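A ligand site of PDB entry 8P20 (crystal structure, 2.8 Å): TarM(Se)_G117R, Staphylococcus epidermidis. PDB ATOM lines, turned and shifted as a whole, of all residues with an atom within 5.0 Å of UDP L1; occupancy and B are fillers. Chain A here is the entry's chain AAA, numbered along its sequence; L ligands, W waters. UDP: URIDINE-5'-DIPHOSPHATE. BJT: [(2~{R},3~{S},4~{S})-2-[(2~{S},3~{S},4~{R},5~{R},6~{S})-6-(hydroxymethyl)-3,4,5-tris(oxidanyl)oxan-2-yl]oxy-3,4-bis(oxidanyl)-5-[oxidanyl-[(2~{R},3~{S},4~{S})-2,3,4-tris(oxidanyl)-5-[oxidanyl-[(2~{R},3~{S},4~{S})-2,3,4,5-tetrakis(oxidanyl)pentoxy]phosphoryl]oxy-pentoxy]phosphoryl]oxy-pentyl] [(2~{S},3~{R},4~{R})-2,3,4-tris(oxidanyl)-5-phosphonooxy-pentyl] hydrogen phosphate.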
ATOM      1  N   LYS A  31      15.025 -21.807   9.992  1.00  0.00           N
ATOM      2  CA  LYS A  31      14.574 -20.469   9.519  1.00  0.00           C
ATOM      3  C   LYS A  31      13.622 -20.636   8.330  1.00  0.00           C
ATOM      4  O   LYS A  31      13.148 -21.764   8.108  1.00  0.00           O
ATOM      5  CB  LYS A  31      15.799 -19.599   9.238  1.00  0.00           C
ATOM      6  CG  LYS A  31      16.582 -19.195  10.472  1.00  0.00           C
ATOM      7  N   GLY A  32      13.345 -19.556   7.589  1.00  0.00           N
ATOM      8  CA  GLY A  32      12.320 -19.515   6.518  1.00  0.00           C
ATOM      9  C   GLY A  32      12.861 -19.000   5.197  1.00  0.00           C
ATOM     10  O   GLY A  32      13.957 -19.435   4.783  1.00  0.00           O
ATOM     11  N   GLY A  33      12.116 -18.090   4.554  1.00  0.00           N
ATOM     12  CA  GLY A  33      12.367 -17.617   3.171  1.00  0.00           C
ATOM     13  C   GLY A  33      13.543 -16.662   3.079  1.00  0.00           C
ATOM     14  O   GLY A  33      14.501 -16.974   2.356  1.00  0.00           O
ATOM     15  N   MET A  34      13.453 -15.515   3.754  1.00  0.00           N
ATOM     16  CA  MET A  34      14.506 -14.465   3.746  1.00  0.00           C
ATOM     17  C   MET A  34      15.887 -15.135   3.776  1.00  0.00           C
ATOM     18  O   MET A  34      16.699 -14.839   2.890  1.00  0.00           O
ATOM     19  CB  MET A  34      14.365 -13.507   4.932  1.00  0.00           C
ATOM     20  CG  MET A  34      15.369 -12.366   4.906  1.00  0.00           C
ATOM     21  SD  MET A  34      15.261 -11.306   6.381  1.00  0.00           S
ATOM     22  CE  MET A  34      13.491 -11.172   6.583  1.00  0.00           C
ATOM     23  N   THR A  36      16.990 -18.351   3.170  1.00  0.00           N
ATOM     24  CA  THR A  36      17.306 -19.150   1.951  1.00  0.00           C
ATOM     25  C   THR A  36      17.603 -18.197   0.787  1.00  0.00           C
ATOM     26  O   THR A  36      18.595 -18.445   0.078  1.00  0.00           O
ATOM     27  CB  THR A  36      16.190 -20.151   1.618  1.00  0.00           C
ATOM     28  OG1 THR A  36      14.927 -19.574   1.970  1.00  0.00           O
ATOM     29  CG2 THR A  36      16.345 -21.479   2.321  1.00  0.00           C
ATOM     30  N   ILE A 340       5.138 -27.004   3.390  1.00  0.00           N
ATOM     31  CA  ILE A 340       6.463 -26.827   4.052  1.00  0.00           C
ATOM     32  C   ILE A 340       6.685 -25.328   4.298  1.00  0.00           C
ATOM     33  O   ILE A 340       7.143 -24.637   3.370  1.00  0.00           O
ATOM     34  CB  ILE A 340       7.596 -27.436   3.199  1.00  0.00           C
ATOM     35  CG1 ILE A 340       7.213 -28.812   2.637  1.00  0.00           C
ATOM     36  CG2 ILE A 340       8.884 -27.506   3.996  1.00  0.00           C
ATOM     37  N   SER A 341       6.349 -24.853   5.496  1.00  0.00           N
ATOM     38  CA  SER A 341       6.517 -23.431   5.903  1.00  0.00           C
ATOM     39  C   SER A 341       6.517 -23.334   7.430  1.00  0.00           C
ATOM     40  O   SER A 341       6.183 -24.332   8.094  1.00  0.00           O
ATOM     41  CB  SER A 341       5.449 -22.567   5.297  1.00  0.00           C
ATOM     42  N   ARG A 342       6.864 -22.156   7.966  1.00  0.00           N
ATOM     43  CA  ARG A 342       6.871 -21.873   9.423  1.00  0.00           C
ATOM     44  C   ARG A 342       5.442 -22.046   9.939  1.00  0.00           C
ATOM     45  O   ARG A 342       4.509 -21.692   9.192  1.00  0.00           O
ATOM     46  CB  ARG A 342       7.395 -20.456   9.693  1.00  0.00           C
ATOM     47  CG  ARG A 342       8.763 -20.160   9.089  1.00  0.00           C
ATOM     48  CD  ARG A 342       9.084 -18.677   9.038  1.00  0.00           C
ATOM     49  NE  ARG A 342       8.110 -17.918   8.251  1.00  0.00           N
ATOM     50  CZ  ARG A 342       7.477 -16.820   8.646  1.00  0.00           C
ATOM     51  NH1 ARG A 342       7.692 -16.299   9.841  1.00  0.00           N
ATOM     52  NH2 ARG A 342       6.611 -16.237   7.828  1.00  0.00           N
ATOM     53  N   GLN A 346       0.903 -15.979   9.664  1.00  0.00           N
ATOM     54  CA  GLN A 346       1.129 -15.527   8.266  1.00  0.00           C
ATOM     55  C   GLN A 346       0.460 -16.507   7.302  1.00  0.00           C
ATOM     56  O   GLN A 346      -0.337 -16.064   6.458  1.00  0.00           O
ATOM     57  CB  GLN A 346       2.626 -15.411   7.971  1.00  0.00           C
ATOM     58  CG  GLN A 346       2.936 -15.217   6.487  1.00  0.00           C
ATOM     59  CD  GLN A 346       4.164 -14.377   6.249  1.00  0.00           C
ATOM     60  OE1 GLN A 346       4.826 -13.927   7.188  1.00  0.00           O
ATOM     61  NE2 GLN A 346       4.489 -14.156   4.990  1.00  0.00           N
ATOM     62  N   LYS A 347       0.744 -17.799   7.465  1.00  0.00           N
ATOM     63  CA  LYS A 347       0.138 -18.898   6.670  1.00  0.00           C
ATOM     64  C   LYS A 347      -1.188 -19.275   7.339  1.00  0.00           C
ATOM     65  O   LYS A 347      -1.171 -19.520   8.553  1.00  0.00           O
ATOM     66  CB  LYS A 347       1.079 -20.105   6.593  1.00  0.00           C
ATOM     67  CG  LYS A 347       2.566 -19.792   6.693  1.00  0.00           C
ATOM     68  CD  LYS A 347       3.193 -19.285   5.412  1.00  0.00           C
ATOM     69  CE  LYS A 347       4.572 -18.673   5.622  1.00  0.00           C
ATOM     70  N   TYR A 371       4.932 -29.650   6.994  1.00  0.00           N
ATOM     71  CA  TYR A 371       6.342 -29.579   7.479  1.00  0.00           C
ATOM     72  C   TYR A 371       6.638 -28.159   7.965  1.00  0.00           C
ATOM     73  O   TYR A 371       5.973 -27.213   7.521  1.00  0.00           O
ATOM     74  CB  TYR A 371       7.315 -30.010   6.385  1.00  0.00           C
ATOM     75  CG  TYR A 371       7.354 -31.492   6.105  1.00  0.00           C
ATOM     76  CD1 TYR A 371       6.409 -32.091   5.290  1.00  0.00           C
ATOM     77  CD2 TYR A 371       8.349 -32.298   6.647  1.00  0.00           C
ATOM     78  CE1 TYR A 371       6.439 -33.454   5.025  1.00  0.00           C
ATOM     79  CE2 TYR A 371       8.393 -33.660   6.392  1.00  0.00           C
ATOM     80  CZ  TYR A 371       7.436 -34.238   5.574  1.00  0.00           C
ATOM     81  OH  TYR A 371       7.472 -35.580   5.330  1.00  0.00           O
ATOM     82  N   GLY A 372       7.645 -28.029   8.848  1.00  0.00           N
ATOM     83  CA  GLY A 372       8.067 -26.746   9.431  1.00  0.00           C
ATOM     84  C   GLY A 372       7.753 -26.679  10.919  1.00  0.00           C
ATOM     85  O   GLY A 372       6.908 -27.475  11.390  1.00  0.00           O
ATOM     86  N   THR A 373       8.413 -25.767  11.639  1.00  0.00           N
ATOM     87  CA  THR A 373       8.222 -25.542  13.095  1.00  0.00           C
ATOM     88  C   THR A 373       7.768 -24.096  13.315  1.00  0.00           C
ATOM     89  O   THR A 373       7.977 -23.274  12.401  1.00  0.00           O
ATOM     90  CB  THR A 373       9.498 -25.894  13.871  1.00  0.00           C
ATOM     91  OG1 THR A 373       9.177 -25.858  15.264  1.00  0.00           O
ATOM     92  CG2 THR A 373      10.647 -24.954  13.586  1.00  0.00           C
ATOM     93  N   GLY A 397       7.280 -31.795  11.196  1.00  0.00           N
ATOM     94  CA  GLY A 397       8.330 -30.939  11.788  1.00  0.00           C
ATOM     95  C   GLY A 397       9.241 -30.360  10.727  1.00  0.00           C
ATOM     96  O   GLY A 397       9.020 -30.627   9.527  1.00  0.00           O
ATOM     97  N   TYR A 398      10.229 -29.554  11.144  1.00  0.00           N
ATOM     98  CA  TYR A 398      11.187 -28.875  10.242  1.00  0.00           C
ATOM     99  C   TYR A 398      11.947 -29.928   9.441  1.00  0.00           C
ATOM    100  O   TYR A 398      12.342 -30.952  10.024  1.00  0.00           O
ATOM    101  CB  TYR A 398      12.151 -27.977  11.003  1.00  0.00           C
ATOM    102  CG  TYR A 398      12.831 -26.947  10.139  1.00  0.00           C
ATOM    103  CD1 TYR A 398      12.250 -25.705   9.924  1.00  0.00           C
ATOM    104  CD2 TYR A 398      14.048 -27.203   9.517  1.00  0.00           C
ATOM    105  CE1 TYR A 398      12.854 -24.756   9.117  1.00  0.00           C
ATOM    106  CE2 TYR A 398      14.664 -26.261   8.713  1.00  0.00           C
ATOM    107  CZ  TYR A 398      14.066 -25.027   8.510  1.00  0.00           C
ATOM    108  OH  TYR A 398      14.665 -24.093   7.719  1.00  0.00           O
ATOM    109  N   THR A 399      12.145 -29.699   8.140  1.00  0.00           N
ATOM    110  CA  THR A 399      12.916 -30.599   7.246  1.00  0.00           C
ATOM    111  C   THR A 399      14.116 -29.819   6.703  1.00  0.00           C
ATOM    112  O   THR A 399      13.921 -28.710   6.166  1.00  0.00           O
ATOM    113  CB  THR A 399      12.041 -31.201   6.144  1.00  0.00           C
ATOM    114  OG1 THR A 399      12.907 -31.830   5.200  1.00  0.00           O
ATOM    115  CG2 THR A 399      11.159 -30.183   5.435  1.00  0.00           C
ATOM    116  N   ALA A 402      13.879 -30.462   2.249  1.00  0.00           N
ATOM    117  CA  ALA A 402      12.486 -30.307   1.767  1.00  0.00           C
ATOM    118  C   ALA A 402      12.381 -30.861   0.345  1.00  0.00           C
ATOM    119  O   ALA A 402      11.301 -31.366  -0.011  1.00  0.00           O
ATOM    120  CB  ALA A 402      12.071 -28.862   1.835  1.00  0.00           C
ATOM    121  N   GLU A 419       2.024 -12.505   2.026  1.00  0.00           N
ATOM    122  CA  GLU A 419       3.339 -13.140   1.701  1.00  0.00           C
ATOM    123  C   GLU A 419       4.145 -12.234   0.765  1.00  0.00           C
ATOM    124  O   GLU A 419       3.628 -11.175   0.368  1.00  0.00           O
ATOM    125  CB  GLU A 419       3.100 -14.511   1.066  1.00  0.00           C
ATOM    126  CG  GLU A 419       3.805 -15.638   1.802  1.00  0.00           C
ATOM    127  CD  GLU A 419       5.326 -15.601   1.719  1.00  0.00           C
ATOM    128  OE1 GLU A 419       5.964 -15.303   2.742  1.00  0.00           O
ATOM    129  OE2 GLU A 419       5.857 -15.873   0.624  1.00  0.00           O
ATOM    130  N   GLY A 422       7.224 -16.127  -2.232  1.00  0.00           N
ATOM    131  CA  GLY A 422       6.679 -17.490  -2.049  1.00  0.00           C
ATOM    132  C   GLY A 422       7.632 -18.545  -2.561  1.00  0.00           C
ATOM    133  O   GLY A 422       7.302 -19.224  -3.558  1.00  0.00           O
ATOM    134  N   LEU A 423       8.777 -18.689  -1.893  1.00  0.00           N
ATOM    135  CA  LEU A 423       9.883 -19.598  -2.306  1.00  0.00           C
ATOM    136  C   LEU A 423       9.408 -21.052  -2.310  1.00  0.00           C
ATOM    137  O   LEU A 423       9.713 -21.762  -3.286  1.00  0.00           O
ATOM    138  CB  LEU A 423      11.076 -19.406  -1.352  1.00  0.00           C
ATOM    139  CG  LEU A 423      11.750 -18.039  -1.418  1.00  0.00           C
ATOM    140  N   SER A 424       8.710 -21.502  -1.265  1.00  0.00           N
ATOM    141  CA  SER A 424       8.312 -22.920  -1.084  1.00  0.00           C
ATOM    142  C   SER A 424       7.451 -23.384  -2.267  1.00  0.00           C
ATOM    143  O   SER A 424       7.619 -24.541  -2.685  1.00  0.00           O
ATOM    144  CB  SER A 424       7.592 -23.146   0.220  1.00  0.00           C
ATOM    145  OG  SER A 424       7.183 -24.506   0.332  1.00  0.00           O
ATOM    146  N   GLU A 427       9.758 -23.508  -5.529  1.00  0.00           N
ATOM    147  CA  GLU A 427      10.621 -24.722  -5.450  1.00  0.00           C
ATOM    148  C   GLU A 427       9.790 -25.952  -5.827  1.00  0.00           C
ATOM    149  O   GLU A 427      10.295 -26.789  -6.594  1.00  0.00           O
ATOM    150  CB  GLU A 427      11.241 -24.876  -4.069  1.00  0.00           C
ATOM    151  CG  GLU A 427      12.269 -23.798  -3.743  1.00  0.00           C
ATOM    152  CD  GLU A 427      12.360 -23.429  -2.278  1.00  0.00           C
ATOM    153  OE1 GLU A 427      11.748 -24.124  -1.445  1.00  0.00           O
ATOM    154  OE2 GLU A 427      13.051 -22.430  -1.964  1.00  0.00           O
HETATM  155  N1  UDP L   1      11.660 -24.158   4.724  1.00  0.00           N
HETATM  156  C2  UDP L   1      12.494 -25.285   4.956  1.00  0.00           C
HETATM  157  N3  UDP L   1      12.161 -26.200   5.866  1.00  0.00           N
HETATM  158  C4  UDP L   1      11.035 -26.060   6.575  1.00  0.00           C
HETATM  159  C5  UDP L   1      10.202 -24.969   6.379  1.00  0.00           C
HETATM  160  C6  UDP L   1      10.546 -24.010   5.437  1.00  0.00           C
HETATM  161  O2  UDP L   1      13.543 -25.442   4.299  1.00  0.00           O
HETATM  162  O4  UDP L   1      10.743 -26.930   7.416  1.00  0.00           O
HETATM  163  C1' UDP L   1      12.051 -23.161   3.732  1.00  0.00           C
HETATM  164  C2' UDP L   1      11.584 -23.535   2.337  1.00  0.00           C
HETATM  165  O2' UDP L   1      12.576 -24.315   1.661  1.00  0.00           O
HETATM  166  C3' UDP L   1      11.366 -22.195   1.668  1.00  0.00           C
HETATM  167  C4' UDP L   1      11.135 -21.229   2.801  1.00  0.00           C
HETATM  168  O4' UDP L   1      11.454 -21.903   4.018  1.00  0.00           O
HETATM  169  O3' UDP L   1      12.545 -21.811   0.962  1.00  0.00           O
HETATM  170  C5' UDP L   1       9.696 -20.718   2.842  1.00  0.00           C
HETATM  171  O5' UDP L   1       9.682 -19.402   2.295  1.00  0.00           O
HETATM  172  PA  UDP L   1       8.307 -18.663   1.910  1.00  0.00           P
HETATM  173  O1A UDP L   1       7.330 -19.706   1.407  1.00  0.00           O
HETATM  174  O2A UDP L   1       8.646 -17.514   0.998  1.00  0.00           O
HETATM  175  O3A UDP L   1       7.708 -18.106   3.317  1.00  0.00           O
HETATM  176  PB  UDP L   1       8.472 -17.157   4.384  1.00  0.00           P
HETATM  177  O1B UDP L   1       9.291 -18.096   5.233  1.00  0.00           O
HETATM  178  O2B UDP L   1       7.341 -16.509   5.142  1.00  0.00           O
HETATM  179  O3B UDP L   1       9.286 -16.172   3.581  1.00  0.00           O
HETATM  180  C4  BJT L   2      11.355  -9.944  14.838  1.00  0.00           C
HETATM  181  C5  BJT L   2      11.986  -9.485  13.532  1.00  0.00           C
HETATM  182  C6  BJT L   2      11.435  -8.129  13.112  1.00  0.00           C
HETATM  183  C3  BJT L   2      11.971 -11.249  15.233  1.00  0.00           C
HETATM  184  OBO BJT L   2      17.889  -3.331  19.979  1.00  0.00           O
HETATM  185  PBN BJT L   2      17.639  -3.322  18.392  1.00  0.00           P
HETATM  186  OCA BJT L   2      19.105  -3.397  17.708  1.00  0.00           O
HETATM  187  OAH BJT L   2      16.872  -2.123  17.973  1.00  0.00           O
HETATM  188  OBM BJT L   2      16.917  -4.702  18.058  1.00  0.00           O
HETATM  189  CBL BJT L   2      15.508  -4.704  17.820  1.00  0.00           C
HETATM  190  CBK BJT L   2      14.988  -6.134  17.734  1.00  0.00           C
HETATM  191  OBZ BJT L   2      13.578  -6.108  17.497  1.00  0.00           O
HETATM  192  CBJ BJT L   2      15.686  -6.920  16.606  1.00  0.00           C
HETATM  193  OAG BJT L   2      15.920  -8.252  17.049  1.00  0.00           O
HETATM  194  CBI BJT L   2      14.824  -6.949  15.344  1.00  0.00           C
HETATM  195  OBY BJT L   2      14.827  -5.659  14.746  1.00  0.00           O
HETATM  196  CBH BJT L   2      15.366  -7.983  14.373  1.00  0.00           C
HETATM  197  OBG BJT L   2      15.766  -7.339  13.181  1.00  0.00           O
HETATM  198  PBF BJT L   2      15.513  -8.029  11.747  1.00  0.00           P
HETATM  199  OBX BJT L   2      16.823  -7.695  10.881  1.00  0.00           O
HETATM  200  OAF BJT L   2      14.277  -7.526  11.112  1.00  0.00           O
HETATM  201  OBE BJT L   2      15.529  -9.602  11.973  1.00  0.00           O
HETATM  202  CBD BJT L   2      14.772 -10.438  11.108  1.00  0.00           C
HETATM  203  CBC BJT L   2      14.571 -11.776  11.808  1.00  0.00           C
HETATM  204  O1  BJT L   2      13.759 -11.593  12.970  1.00  0.00           O
HETATM  205  C1  BJT L   2      12.318 -11.713  12.826  1.00  0.00           C
HETATM  206  O5  BJT L   2      11.716 -10.446  12.507  1.00  0.00           O
HETATM  207  O6  BJT L   2      10.053  -8.047  13.453  1.00  0.00           O
HETATM  208  O4  BJT L   2      11.600  -8.962  15.849  1.00  0.00           O
HETATM  209  O3  BJT L   2      11.358 -11.725  16.422  1.00  0.00           O
HETATM  210  C2  BJT L   2      11.748 -12.249  14.118  1.00  0.00           C
HETATM  211  O2  BJT L   2      12.404 -13.480  14.444  1.00  0.00           O
HETATM  212  CBB BJT L   2      13.983 -12.797  10.833  1.00  0.00           C
HETATM  213  OAE BJT L   2      13.187 -12.149   9.833  1.00  0.00           O
HETATM  214  CBA BJT L   2      15.124 -13.539  10.135  1.00  0.00           C
HETATM  215  OBV BJT L   2      16.197 -13.736  11.045  1.00  0.00           O
HETATM  216  CAZ BJT L   2      14.637 -14.906   9.679  1.00  0.00           C
HETATM  217  OAY BJT L   2      13.921 -14.758   8.460  1.00  0.00           O
HETATM  218  PAX BJT L   2      13.127 -16.024   7.893  1.00  0.00           P
HETATM  219  OBU BJT L   2      13.185 -17.172   9.047  1.00  0.00           O
HETATM  220  OAD BJT L   2      13.751 -16.529   6.643  1.00  0.00           O
HETATM  221  OAW BJT L   2      11.597 -15.587   7.804  1.00  0.00           O
HETATM  222  CAV BJT L   2      11.016 -15.169   6.568  1.00  0.00           C
HETATM  223  CAU BJT L   2      10.522 -13.727   6.688  1.00  0.00           C
HETATM  224  OBT BJT L   2      10.206 -13.227   5.398  1.00  0.00           O
HETATM  225  CAT BJT L   2       9.287 -13.686   7.582  1.00  0.00           C
HETATM  226  OAC BJT L   2       9.682 -13.736   8.954  1.00  0.00           O
HETATM  227  CAS BJT L   2       8.540 -12.395   7.337  1.00  0.00           C
HETATM  228  OBS BJT L   2       7.638 -12.572   6.244  1.00  0.00           O
HETATM  229  CAR BJT L   2       7.751 -12.046   8.587  1.00  0.00           C
HETATM  230  OAQ BJT L   2       6.657 -11.207   8.239  1.00  0.00           O
HETATM  231  PAP BJT L   2       6.363  -9.884   9.116  1.00  0.00           P
HETATM  232  OBR BJT L   2       4.864  -9.442   8.714  1.00  0.00           O
HETATM  233  OAB BJT L   2       7.380  -8.841   8.882  1.00  0.00           O
HETATM  234  OAO BJT L   2       6.357 -10.368  10.653  1.00  0.00           O
HETATM  235  CAN BJT L   2       5.152 -10.597  11.387  1.00  0.00           C
HETATM  236  CAM BJT L   2       5.240  -9.819  12.697  1.00  0.00           C
HETATM  237  OBQ BJT L   2       6.460 -10.167  13.357  1.00  0.00           O
HETATM  238  CAL BJT L   2       5.253  -8.303  12.459  1.00  0.00           C
HETATM  239  OAA BJT L   2       4.446  -7.947  11.334  1.00  0.00           O
HETATM  240  CAK BJT L   2       4.706  -7.605  13.700  1.00  0.00           C
HETATM  241  OBP BJT L   2       5.515  -7.939  14.833  1.00  0.00           O
HETATM  242  CAJ BJT L   2       4.720  -6.083  13.500  1.00  0.00           C
HETATM  243  OAI BJT L   2       3.539  -5.690  12.800  1.00  0.00           O
HETATM  244  O   HOH W   1      14.566 -21.996   5.629  1.00  0.00           O
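The guanidinium group (NH2) of Arg 342 is in salt-bridge range of an oxygen (O2B) of UDP L1.
An oxygen (O1B) of UDP L1 is in hydrogen-bond range of the backbone NH (N) of Gly 33.
O2B of UDP L1 lies close to OE1 of Glu 419.
An oxygen (O3') of UDP L1 is in hydrogen-bond range of the side-chain carboxylate (OE2) of Glu 427 (3.0 Å).
The backbone NH (N) of Thr 399 lies within hydrogen-bond range of an oxygen (O4) of UDP L1.
N3 of UDP L1 lies within hydrogen-bond range of O of Thr 399.
The backbone NH (N) of Leu 423 sits at hydrogen-bond distance from an oxygen (O2A) of UDP L1, at 3.1 Å.
The side-chain hydroxyl (OG1) of Thr 36 is in hydrogen-bond range of an oxygen (O3') of UDP L1, 3.4 Å away.
NH1 of Arg 342 is in hydrogen-bond range of OAC of BJT L2, 3.4 Å away.
OAD of BJT L2 lies within hydrogen-bond range of N of Gly 33.
The backbone NH (N) of Gly 32 is in hydrogen-bond range of an oxygen (OBU) of BJT L2.
The side-chain amide oxygen (OE1) of Gln 346 sits at hydrogen-bond distance from an oxygen (OBS) of BJT L2 (3.3 Å).
N of Met 34 is in hydrogen-bond range of OAD of BJT L2, 3.1 Å away.
The guanidinium group of Arg 342 sits at hydrogen-bond distance from the side-chain amide oxygen of Gln 346, at 3.0 Å.
O of Gly 33 sits at hydrogen-bond distance from OG1 of Thr 36.
The backbone NH of Gly 422 lies within hydrogen-bond range of the side-chain carboxylate of Glu 419 (3.2 Å).
OE1 of Glu 419 lies within hydrogen-bond range of NE2 of Gln 346 (2.9 Å).
The side-chain hydroxyl (OG1) of Thr 399 lies within hydrogen-bond range of the backbone NH (N) of Ala 402.
N of Gly 372 lies within hydrogen-bond range of O of Gly 397 (3.0 Å).
The backbone carbonyl oxygen of Ile 340 sits at hydrogen-bond distance from the side-chain hydroxyl of Ser 424, 3.0 Å away.
O of Tyr 371 sits at hydrogen-bond distance from N of Ser 341 (3.1 Å).
Gly 32 touches UDP L1 (C to O4', 3.4 Å).
Ile 340 touches UDP L1.
N of Ser 341 touches C5 of UDP L1, at 3.95 Å.
Gln 346 touches UDP L1.
CE of Lys 347 touches O2B of UDP L1 (3.5 Å).
Gly 372 touches UDP L1.
Tyr 398 touches UDP L1 (CD1 to O4, 3.2 Å).
Gly 422 touches UDP L1 (CA to O2A, 3.6 Å).
Ser 424 touches UDP L1.
Hydrophobic or aromatic side chains within 4 Å of UDP L1: Ile 340, Tyr 398 and Leu 423.
Along chain A the residues within 4 Å of UDP L1 span positions 32 to 427.
Water W1 lies within hydrogen-bond range of the backbone carbonyl oxygen of Gly 32 (2.8 Å), the backbone carbonyl oxygen of Lys 31 (2.9 Å) and the side-chain hydroxyl of Tyr 398 (3.0 Å).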
